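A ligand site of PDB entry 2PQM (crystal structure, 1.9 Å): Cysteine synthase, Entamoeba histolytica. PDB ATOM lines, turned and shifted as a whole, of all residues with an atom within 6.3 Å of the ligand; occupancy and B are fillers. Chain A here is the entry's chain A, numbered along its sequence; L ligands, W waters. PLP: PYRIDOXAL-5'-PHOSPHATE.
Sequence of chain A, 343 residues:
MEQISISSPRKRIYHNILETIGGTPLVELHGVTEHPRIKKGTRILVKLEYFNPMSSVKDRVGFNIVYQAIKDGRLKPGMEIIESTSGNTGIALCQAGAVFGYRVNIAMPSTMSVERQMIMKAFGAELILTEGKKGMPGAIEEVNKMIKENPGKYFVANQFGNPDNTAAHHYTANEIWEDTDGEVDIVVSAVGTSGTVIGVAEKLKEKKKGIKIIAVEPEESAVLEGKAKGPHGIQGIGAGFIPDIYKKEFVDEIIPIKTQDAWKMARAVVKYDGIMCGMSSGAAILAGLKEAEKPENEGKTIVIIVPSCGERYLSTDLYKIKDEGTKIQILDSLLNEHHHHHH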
ATOM      1  N   SER A  56     -18.378 -13.415 -17.885  1.00  0.00           N
ATOM      2  CA  SER A  56     -18.137 -13.456 -19.336  1.00  0.00           C
ATOM      3  C   SER A  56     -19.246 -12.790 -20.127  1.00  0.00           C
ATOM      4  O   SER A  56     -20.370 -12.653 -19.637  1.00  0.00           O
ATOM      5  CB  SER A  56     -17.915 -14.890 -19.862  1.00  0.00           C
ATOM      6  OG  SER A  56     -19.130 -15.543 -20.227  1.00  0.00           O
ATOM      7  N   VAL A  57     -18.906 -12.426 -21.369  1.00  0.00           N
ATOM      8  CA  VAL A  57     -19.839 -11.927 -22.363  1.00  0.00           C
ATOM      9  C   VAL A  57     -21.082 -12.824 -22.526  1.00  0.00           C
ATOM     10  O   VAL A  57     -22.148 -12.315 -22.872  1.00  0.00           O
ATOM     11  CB  VAL A  57     -19.110 -11.726 -23.729  1.00  0.00           C
ATOM     12  CG1 VAL A  57     -18.638 -13.093 -24.315  1.00  0.00           C
ATOM     13  CG2 VAL A  57     -19.984 -10.943 -24.728  1.00  0.00           C
ATOM     14  N   LYS A  58     -20.957 -14.128 -22.273  1.00  0.00           N
ATOM     15  CA  LYS A  58     -22.086 -15.058 -22.576  1.00  0.00           C
ATOM     16  C   LYS A  58     -23.246 -14.862 -21.628  1.00  0.00           C
ATOM     17  O   LYS A  58     -24.366 -15.336 -21.906  1.00  0.00           O
ATOM     18  CB  LYS A  58     -21.627 -16.527 -22.538  1.00  0.00           C
ATOM     19  CG  LYS A  58     -20.561 -16.861 -23.546  1.00  0.00           C
ATOM     20  CD  LYS A  58     -21.053 -16.572 -24.976  1.00  0.00           C
ATOM     21  CE  LYS A  58     -20.303 -17.470 -25.957  1.00  0.00           C
ATOM     22  NZ  LYS A  58     -18.866 -17.244 -25.719  1.00  0.00           N
ATOM     23  N   VAL A  61     -25.899 -13.534 -23.534  1.00  0.00           N
ATOM     24  CA  VAL A  61     -26.410 -14.509 -24.516  1.00  0.00           C
ATOM     25  C   VAL A  61     -27.337 -15.538 -23.860  1.00  0.00           C
ATOM     26  O   VAL A  61     -28.452 -15.765 -24.324  1.00  0.00           O
ATOM     27  CB  VAL A  61     -25.227 -15.179 -25.238  1.00  0.00           C
ATOM     28  CG1 VAL A  61     -25.700 -16.263 -26.248  1.00  0.00           C
ATOM     29  CG2 VAL A  61     -24.380 -14.116 -25.931  1.00  0.00           C
ATOM     30  N   GLY A  87     -18.159 -24.403 -22.519  1.00  0.00           N
ATOM     31  CA  GLY A  87     -17.671 -23.048 -22.215  1.00  0.00           C
ATOM     32  C   GLY A  87     -18.623 -22.191 -21.401  1.00  0.00           C
ATOM     33  O   GLY A  87     -19.508 -22.667 -20.648  1.00  0.00           O
ATOM     34  N   ASN A  88     -18.432 -20.889 -21.585  1.00  0.00           N
ATOM     35  CA  ASN A  88     -19.152 -19.861 -20.861  1.00  0.00           C
ATOM     36  C   ASN A  88     -20.654 -19.884 -21.123  1.00  0.00           C
ATOM     37  O   ASN A  88     -21.450 -19.509 -20.252  1.00  0.00           O
ATOM     38  CB  ASN A  88     -18.563 -18.512 -21.251  1.00  0.00           C
ATOM     39  CG  ASN A  88     -17.161 -18.301 -20.683  1.00  0.00           C
ATOM     40  OD1 ASN A  88     -16.283 -17.669 -21.324  1.00  0.00           O
ATOM     41  ND2 ASN A  88     -16.957 -18.780 -19.477  1.00  0.00           N
ATOM     42  N   THR A  89     -21.053 -20.305 -22.311  1.00  0.00           N
ATOM     43  CA  THR A  89     -22.510 -20.295 -22.618  1.00  0.00           C
ATOM     44  C   THR A  89     -23.234 -21.230 -21.645  1.00  0.00           C
ATOM     45  O   THR A  89     -24.322 -20.907 -21.180  1.00  0.00           O
ATOM     46  CB  THR A  89     -22.750 -20.640 -24.087  1.00  0.00           C
ATOM     47  OG1 THR A  89     -22.290 -19.544 -24.882  1.00  0.00           O
ATOM     48  CG2 THR A  89     -24.271 -20.823 -24.383  1.00  0.00           C
ATOM     49  N   GLN A 159     -26.545 -21.777 -29.709  1.00  0.00           N
ATOM     50  CA  GLN A 159     -25.803 -20.503 -29.670  1.00  0.00           C
ATOM     51  C   GLN A 159     -25.241 -19.967 -31.005  1.00  0.00           C
ATOM     52  O   GLN A 159     -25.173 -18.756 -31.217  1.00  0.00           O
ATOM     53  CB  GLN A 159     -24.714 -20.579 -28.582  1.00  0.00           C
ATOM     54  CG  GLN A 159     -23.615 -21.558 -28.873  1.00  0.00           C
ATOM     55  CD  GLN A 159     -22.493 -21.500 -27.838  1.00  0.00           C
ATOM     56  OE1 GLN A 159     -22.171 -20.414 -27.334  1.00  0.00           O
ATOM     57  NE2 GLN A 159     -21.937 -22.652 -27.495  1.00  0.00           N
ATOM     58  N   ASN A 165     -28.934 -14.364 -29.840  1.00  0.00           N
ATOM     59  CA  ASN A 165     -27.529 -14.169 -29.464  1.00  0.00           C
ATOM     60  C   ASN A 165     -27.074 -12.792 -30.043  1.00  0.00           C
ATOM     61  O   ASN A 165     -26.772 -11.838 -29.281  1.00  0.00           O
ATOM     62  CB  ASN A 165     -26.703 -15.372 -29.975  1.00  0.00           C
ATOM     63  CG  ASN A 165     -25.188 -15.210 -29.719  1.00  0.00           C
ATOM     64  OD1 ASN A 165     -24.695 -14.118 -29.399  1.00  0.00           O
ATOM     65  ND2 ASN A 165     -24.433 -16.289 -29.915  1.00  0.00           N
ATOM     66  N   HIS A 169     -26.488  -8.219 -28.416  1.00  0.00           N
ATOM     67  CA  HIS A 169     -25.376  -7.289 -28.615  1.00  0.00           C
ATOM     68  C   HIS A 169     -25.733  -5.913 -29.158  1.00  0.00           C
ATOM     69  O   HIS A 169     -24.877  -5.019 -29.290  1.00  0.00           O
ATOM     70  CB  HIS A 169     -24.257  -7.990 -29.357  1.00  0.00           C
ATOM     71  CG  HIS A 169     -23.635  -9.059 -28.529  1.00  0.00           C
ATOM     72  ND1 HIS A 169     -22.870  -8.764 -27.419  1.00  0.00           N
ATOM     73  CD2 HIS A 169     -23.746 -10.402 -28.581  1.00  0.00           C
ATOM     74  CE1 HIS A 169     -22.474  -9.893 -26.863  1.00  0.00           C
ATOM     75  NE2 HIS A 169     -23.020 -10.904 -27.533  1.00  0.00           N
ATOM     76  N   SER A 189     -13.412  -7.334 -32.278  1.00  0.00           N
ATOM     77  CA  SER A 189     -14.055  -8.451 -31.565  1.00  0.00           C
ATOM     78  C   SER A 189     -13.513  -9.777 -32.050  1.00  0.00           C
ATOM     79  O   SER A 189     -13.600 -10.080 -33.259  1.00  0.00           O
ATOM     80  CB  SER A 189     -15.577  -8.387 -31.755  1.00  0.00           C
ATOM     81  OG  SER A 189     -16.256  -9.556 -31.279  1.00  0.00           O
ATOM     82  N   ALA A 190     -12.959 -10.577 -31.118  1.00  0.00           N
ATOM     83  CA  ALA A 190     -12.580 -11.970 -31.404  1.00  0.00           C
ATOM     84  C   ALA A 190     -13.829 -12.844 -31.518  1.00  0.00           C
ATOM     85  O   ALA A 190     -14.712 -12.810 -30.653  1.00  0.00           O
ATOM     86  CB  ALA A 190     -11.671 -12.492 -30.301  1.00  0.00           C
ATOM     87  N   VAL A 191     -13.872 -13.678 -32.556  1.00  0.00           N
ATOM     88  CA  VAL A 191     -15.111 -14.307 -32.938  1.00  0.00           C
ATOM     89  C   VAL A 191     -15.218 -15.768 -32.473  1.00  0.00           C
ATOM     90  O   VAL A 191     -14.393 -16.591 -32.865  1.00  0.00           O
ATOM     91  CB  VAL A 191     -15.297 -14.237 -34.493  1.00  0.00           C
ATOM     92  CG1 VAL A 191     -16.484 -15.141 -34.950  1.00  0.00           C
ATOM     93  CG2 VAL A 191     -15.438 -12.774 -34.951  1.00  0.00           C
ATOM     94  N   GLY A 192     -16.254 -16.054 -31.678  1.00  0.00           N
ATOM     95  CA  GLY A 192     -16.650 -17.427 -31.292  1.00  0.00           C
ATOM     96  C   GLY A 192     -17.931 -17.765 -32.065  1.00  0.00           C
ATOM     97  O   GLY A 192     -17.874 -18.324 -33.172  1.00  0.00           O
ATOM     98  N   THR A 193     -19.076 -17.410 -31.490  1.00  0.00           N
ATOM     99  CA  THR A 193     -20.387 -17.507 -32.161  1.00  0.00           C
ATOM    100  C   THR A 193     -20.599 -16.414 -33.221  1.00  0.00           C
ATOM    101  O   THR A 193     -21.428 -16.560 -34.137  1.00  0.00           O
ATOM    102  CB  THR A 193     -21.559 -17.429 -31.147  1.00  0.00           C
ATOM    103  OG1 THR A 193     -21.609 -16.114 -30.552  1.00  0.00           O
ATOM    104  CG2 THR A 193     -21.436 -18.475 -30.065  1.00  0.00           C
ATOM    105  N   SER A 194     -19.836 -15.313 -33.066  1.00  0.00           N
ATOM    106  CA  SER A 194     -19.998 -14.047 -33.812  1.00  0.00           C
ATOM    107  C   SER A 194     -21.192 -13.188 -33.347  1.00  0.00           C
ATOM    108  O   SER A 194     -21.428 -12.149 -33.951  1.00  0.00           O
ATOM    109  CB  SER A 194     -20.039 -14.215 -35.357  1.00  0.00           C
ATOM    110  OG  SER A 194     -21.317 -14.677 -35.817  1.00  0.00           O
ATOM    111  N   GLY A 195     -21.912 -13.583 -32.304  1.00  0.00           N
ATOM    112  CA  GLY A 195     -22.967 -12.716 -31.754  1.00  0.00           C
ATOM    113  C   GLY A 195     -22.452 -11.285 -31.521  1.00  0.00           C
ATOM    114  O   GLY A 195     -23.079 -10.295 -31.908  1.00  0.00           O
ATOM    115  N   THR A 196     -21.284 -11.175 -30.897  1.00  0.00           N
ATOM    116  CA  THR A 196     -20.779  -9.850 -30.497  1.00  0.00           C
ATOM    117  C   THR A 196     -20.432  -8.980 -31.707  1.00  0.00           C
ATOM    118  O   THR A 196     -20.924  -7.873 -31.832  1.00  0.00           O
ATOM    119  CB  THR A 196     -19.545  -9.945 -29.534  1.00  0.00           C
ATOM    120  OG1 THR A 196     -19.887 -10.758 -28.407  1.00  0.00           O
ATOM    121  CG2 THR A 196     -19.145  -8.558 -29.014  1.00  0.00           C
ATOM    122  N   VAL A 197     -19.589  -9.475 -32.604  1.00  0.00           N
ATOM    123  CA  VAL A 197     -19.121  -8.622 -33.709  1.00  0.00           C
ATOM    124  C   VAL A 197     -20.304  -8.240 -34.630  1.00  0.00           C
ATOM    125  O   VAL A 197     -20.417  -7.095 -35.034  1.00  0.00           O
ATOM    126  CB  VAL A 197     -17.965  -9.290 -34.508  1.00  0.00           C
ATOM    127  CG1 VAL A 197     -18.474 -10.505 -35.333  1.00  0.00           C
ATOM    128  CG2 VAL A 197     -17.249  -8.240 -35.387  1.00  0.00           C
ATOM    129  N   GLN A 235      -8.756 -20.339 -26.465  1.00  0.00           N
ATOM    130  CA  GLN A 235     -10.034 -20.795 -25.957  1.00  0.00           C
ATOM    131  C   GLN A 235     -11.106 -19.722 -26.155  1.00  0.00           C
ATOM    132  O   GLN A 235     -10.830 -18.515 -25.953  1.00  0.00           O
ATOM    133  CB  GLN A 235      -9.927 -21.107 -24.474  1.00  0.00           C
ATOM    134  CG  GLN A 235      -9.281 -22.396 -24.127  1.00  0.00           C
ATOM    135  CD  GLN A 235      -9.667 -22.839 -22.715  1.00  0.00           C
ATOM    136  OE1 GLN A 235     -10.432 -22.159 -22.009  1.00  0.00           O
ATOM    137  NE2 GLN A 235      -9.161 -23.970 -22.301  1.00  0.00           N
ATOM    138  N   GLY A 236     -12.300 -20.156 -26.550  1.00  0.00           N
ATOM    139  CA  GLY A 236     -13.486 -19.306 -26.674  1.00  0.00           C
ATOM    140  C   GLY A 236     -13.704 -18.769 -28.080  1.00  0.00           C
ATOM    141  O   GLY A 236     -14.792 -18.235 -28.401  1.00  0.00           O
ATOM    142  N   ILE A 237     -12.686 -18.908 -28.935  1.00  0.00           N
ATOM    143  CA  ILE A 237     -12.857 -18.511 -30.333  1.00  0.00           C
ATOM    144  C   ILE A 237     -12.403 -19.641 -31.263  1.00  0.00           C
ATOM    145  O   ILE A 237     -12.046 -20.725 -30.788  1.00  0.00           O
ATOM    146  CB  ILE A 237     -12.169 -17.147 -30.686  1.00  0.00           C
ATOM    147  CG1 ILE A 237     -10.630 -17.259 -30.633  1.00  0.00           C
ATOM    148  CG2 ILE A 237     -12.717 -15.982 -29.776  1.00  0.00           C
ATOM    149  CD1 ILE A 237      -9.945 -16.067 -31.333  1.00  0.00           C
ATOM    150  N   SER A 280      -8.796 -15.065 -25.430  1.00  0.00           N
ATOM    151  CA  SER A 280      -9.380 -14.429 -26.613  1.00  0.00           C
ATOM    152  C   SER A 280      -9.210 -12.893 -26.541  1.00  0.00           C
ATOM    153  O   SER A 280      -9.103 -12.199 -27.570  1.00  0.00           O
ATOM    154  CB  SER A 280     -10.837 -14.831 -26.742  1.00  0.00           C
ATOM    155  OG  SER A 280     -11.638 -14.278 -25.689  1.00  0.00           O
ATOM    156  N   SER A 281      -9.224 -12.369 -25.312  1.00  0.00           N
ATOM    157  CA  SER A 281      -8.924 -10.932 -25.088  1.00  0.00           C
ATOM    158  C   SER A 281      -7.518 -10.547 -25.517  1.00  0.00           C
ATOM    159  O   SER A 281      -7.298  -9.452 -26.030  1.00  0.00           O
ATOM    160  CB  SER A 281      -9.107 -10.525 -23.618  1.00  0.00           C
ATOM    161  OG  SER A 281     -10.421 -10.773 -23.171  1.00  0.00           O
ATOM    162  N   PRO A 307     -13.806 -10.498 -23.681  1.00  0.00           N
ATOM    163  CA  PRO A 307     -14.894 -11.417 -23.326  1.00  0.00           C
ATOM    164  C   PRO A 307     -14.839 -12.098 -21.952  1.00  0.00           C
ATOM    165  O   PRO A 307     -15.877 -12.515 -21.474  1.00  0.00           O
ATOM    166  CB  PRO A 307     -14.836 -12.463 -24.434  1.00  0.00           C
ATOM    167  CG  PRO A 307     -14.218 -11.708 -25.598  1.00  0.00           C
ATOM    168  CD  PRO A 307     -13.101 -10.988 -24.878  1.00  0.00           C
ATOM    169  N   SER A 308     -13.667 -12.233 -21.344  1.00  0.00           N
ATOM    170  CA  SER A 308     -13.493 -13.092 -20.151  1.00  0.00           C
ATOM    171  C   SER A 308     -12.259 -12.714 -19.317  1.00  0.00           C
ATOM    172  O   SER A 308     -11.413 -11.969 -19.798  1.00  0.00           O
ATOM    173  CB  SER A 308     -13.395 -14.572 -20.554  1.00  0.00           C
ATOM    174  OG  SER A 308     -12.133 -14.838 -21.175  1.00  0.00           O
ATOM    175  N   TYR A 313      -8.624 -19.435 -16.526  1.00  0.00           N
ATOM    176  CA  TYR A 313      -7.592 -20.043 -17.382  1.00  0.00           C
ATOM    177  C   TYR A 313      -6.394 -20.573 -16.613  1.00  0.00           C
ATOM    178  O   TYR A 313      -5.362 -20.890 -17.211  1.00  0.00           O
ATOM    179  CB  TYR A 313      -7.107 -19.008 -18.414  1.00  0.00           C
ATOM    180  CG  TYR A 313      -8.261 -18.569 -19.281  1.00  0.00           C
ATOM    181  CD1 TYR A 313      -8.551 -19.223 -20.486  1.00  0.00           C
ATOM    182  CD2 TYR A 313      -9.105 -17.529 -18.865  1.00  0.00           C
ATOM    183  CE1 TYR A 313      -9.654 -18.821 -21.271  1.00  0.00           C
ATOM    184  CE2 TYR A 313     -10.197 -17.119 -19.648  1.00  0.00           C
ATOM    185  CZ  TYR A 313     -10.470 -17.765 -20.831  1.00  0.00           C
ATOM    186  OH  TYR A 313     -11.555 -17.364 -21.551  1.00  0.00           O
HETATM  187  N1  PLP L   1     -14.020 -15.332 -25.806  1.00  0.00           N
HETATM  188  C2  PLP L   1     -14.686 -16.053 -24.846  1.00  0.00           C
HETATM  189  C2A PLP L   1     -13.935 -16.493 -23.604  1.00  0.00           C
HETATM  190  C3  PLP L   1     -16.018 -16.409 -25.098  1.00  0.00           C
HETATM  191  O3  PLP L   1     -16.747 -17.110 -24.170  1.00  0.00           O
HETATM  192  C4  PLP L   1     -16.620 -15.973 -26.312  1.00  0.00           C
HETATM  193  C4A PLP L   1     -18.031 -16.347 -26.598  1.00  0.00           C
HETATM  194  C5  PLP L   1     -15.917 -15.197 -27.259  1.00  0.00           C
HETATM  195  C6  PLP L   1     -14.589 -14.901 -26.983  1.00  0.00           C
HETATM  196  C5A PLP L   1     -16.453 -14.787 -28.623  1.00  0.00           C
HETATM  197  O4P PLP L   1     -17.645 -14.010 -28.509  1.00  0.00           O
HETATM  198  P   PLP L   1     -18.818 -14.255 -29.604  1.00  0.00           P
HETATM  199  O1P PLP L   1     -19.840 -13.180 -29.416  1.00  0.00           O
HETATM  200  O2P PLP L   1     -18.159 -14.152 -30.956  1.00  0.00           O
HETATM  201  O3P PLP L   1     -19.391 -15.652 -29.391  1.00  0.00           O
HETATM  202  O   HOH W   1     -22.281 -13.614 -28.043  1.00  0.00           O
HETATM  203  O   HOH W   2     -17.445 -11.515 -27.327  1.00  0.00           O
HETATM  204  O   HOH W   3     -16.507 -19.674 -23.995  1.00  0.00           O
HETATM  205  O   HOH W   4     -17.894 -11.816 -32.187  1.00  0.00           O
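The side-chain amino group (NZ) of Lys 58 is covalently linked to a carbon (C4A) of the ligand, 1.5 Å away. O3P of the ligand is in hydrogen-bond range of N of Thr 193 (2.8 Å). The side-chain hydroxyl of Thr 193 sits at hydrogen-bond distance from an oxygen (O3P) of the ligand (2.5 Å). OG of Ser 280 sits at hydrogen-bond distance from N1 of the ligand. N of Thr 196 lies within hydrogen-bond range of O1P of the ligand. The side-chain hydroxyl of Thr 196 lies within hydrogen-bond range of an oxygen (O1P) of the ligand (2.6 Å). N of Gly 192 lies within hydrogen-bond range of O2P of the ligand (2.8 Å). O2P of the ligand lies within hydrogen-bond range of N of Ser 194, at 2.9 Å. An oxygen (O3) of the ligand lies within hydrogen-bond range of the side-chain amide oxygen (OD1) of Asn 88 (2.9 Å).
N of Lys 58 sits close to OG of Ser 56. N of Gly 195 is in hydrogen-bond range of OG1 of Thr 193 (3.1 Å). OG1 of Thr 193 sits at hydrogen-bond distance from ND2 of Asn 165. OG1 of Thr 196 lies close to NE2 of His 169 (3.3 Å). OG of Ser 308 lies within hydrogen-bond range of OH of Tyr 313 (2.6 Å). The backbone carbonyl oxygen (O) of Pro 307 is in hydrogen-bond range of the backbone NH (N) of Val 57, 3.0 Å away.
Residues that only touch the ligand: Ala 190 (3.3 Å), Val 191 (3.6 Å), Gly 195 (3.6 Å), Gly 236 (3.4 Å), Ile 237 (3.5 Å), Pro 307 (3.3 Å), Ser 308 (3.4 Å) and Tyr 313 (3.3 Å). Hydrophobic or aromatic side chains within 4 Å of the ligand: Ile 237 and Pro 307. Along chain A the residues within 4 Å of the ligand span positions 58 to 313.
Water W3 lies within hydrogen-bond range of O3 of the ligand and N of Asn 88. Water W4 lies within hydrogen-bond range of an oxygen (O2P) of the ligand (2.7 Å), the backbone NH (N) of Val 197 (2.9 Å) and the side-chain hydroxyl (OG) of Ser 189 (2.9 Å). Water W2 bridges O4P of the ligand (2.8 Å) and OG1 of Thr 196 (2.8 Å). Water W1 lies within hydrogen-bond range of the side-chain amide oxygen of Asn 165 (2.8 Å), an oxygen (O1P) of the ligand (2.8 Å) and a ring nitrogen (NE2) of His 169 (2.9 Å).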
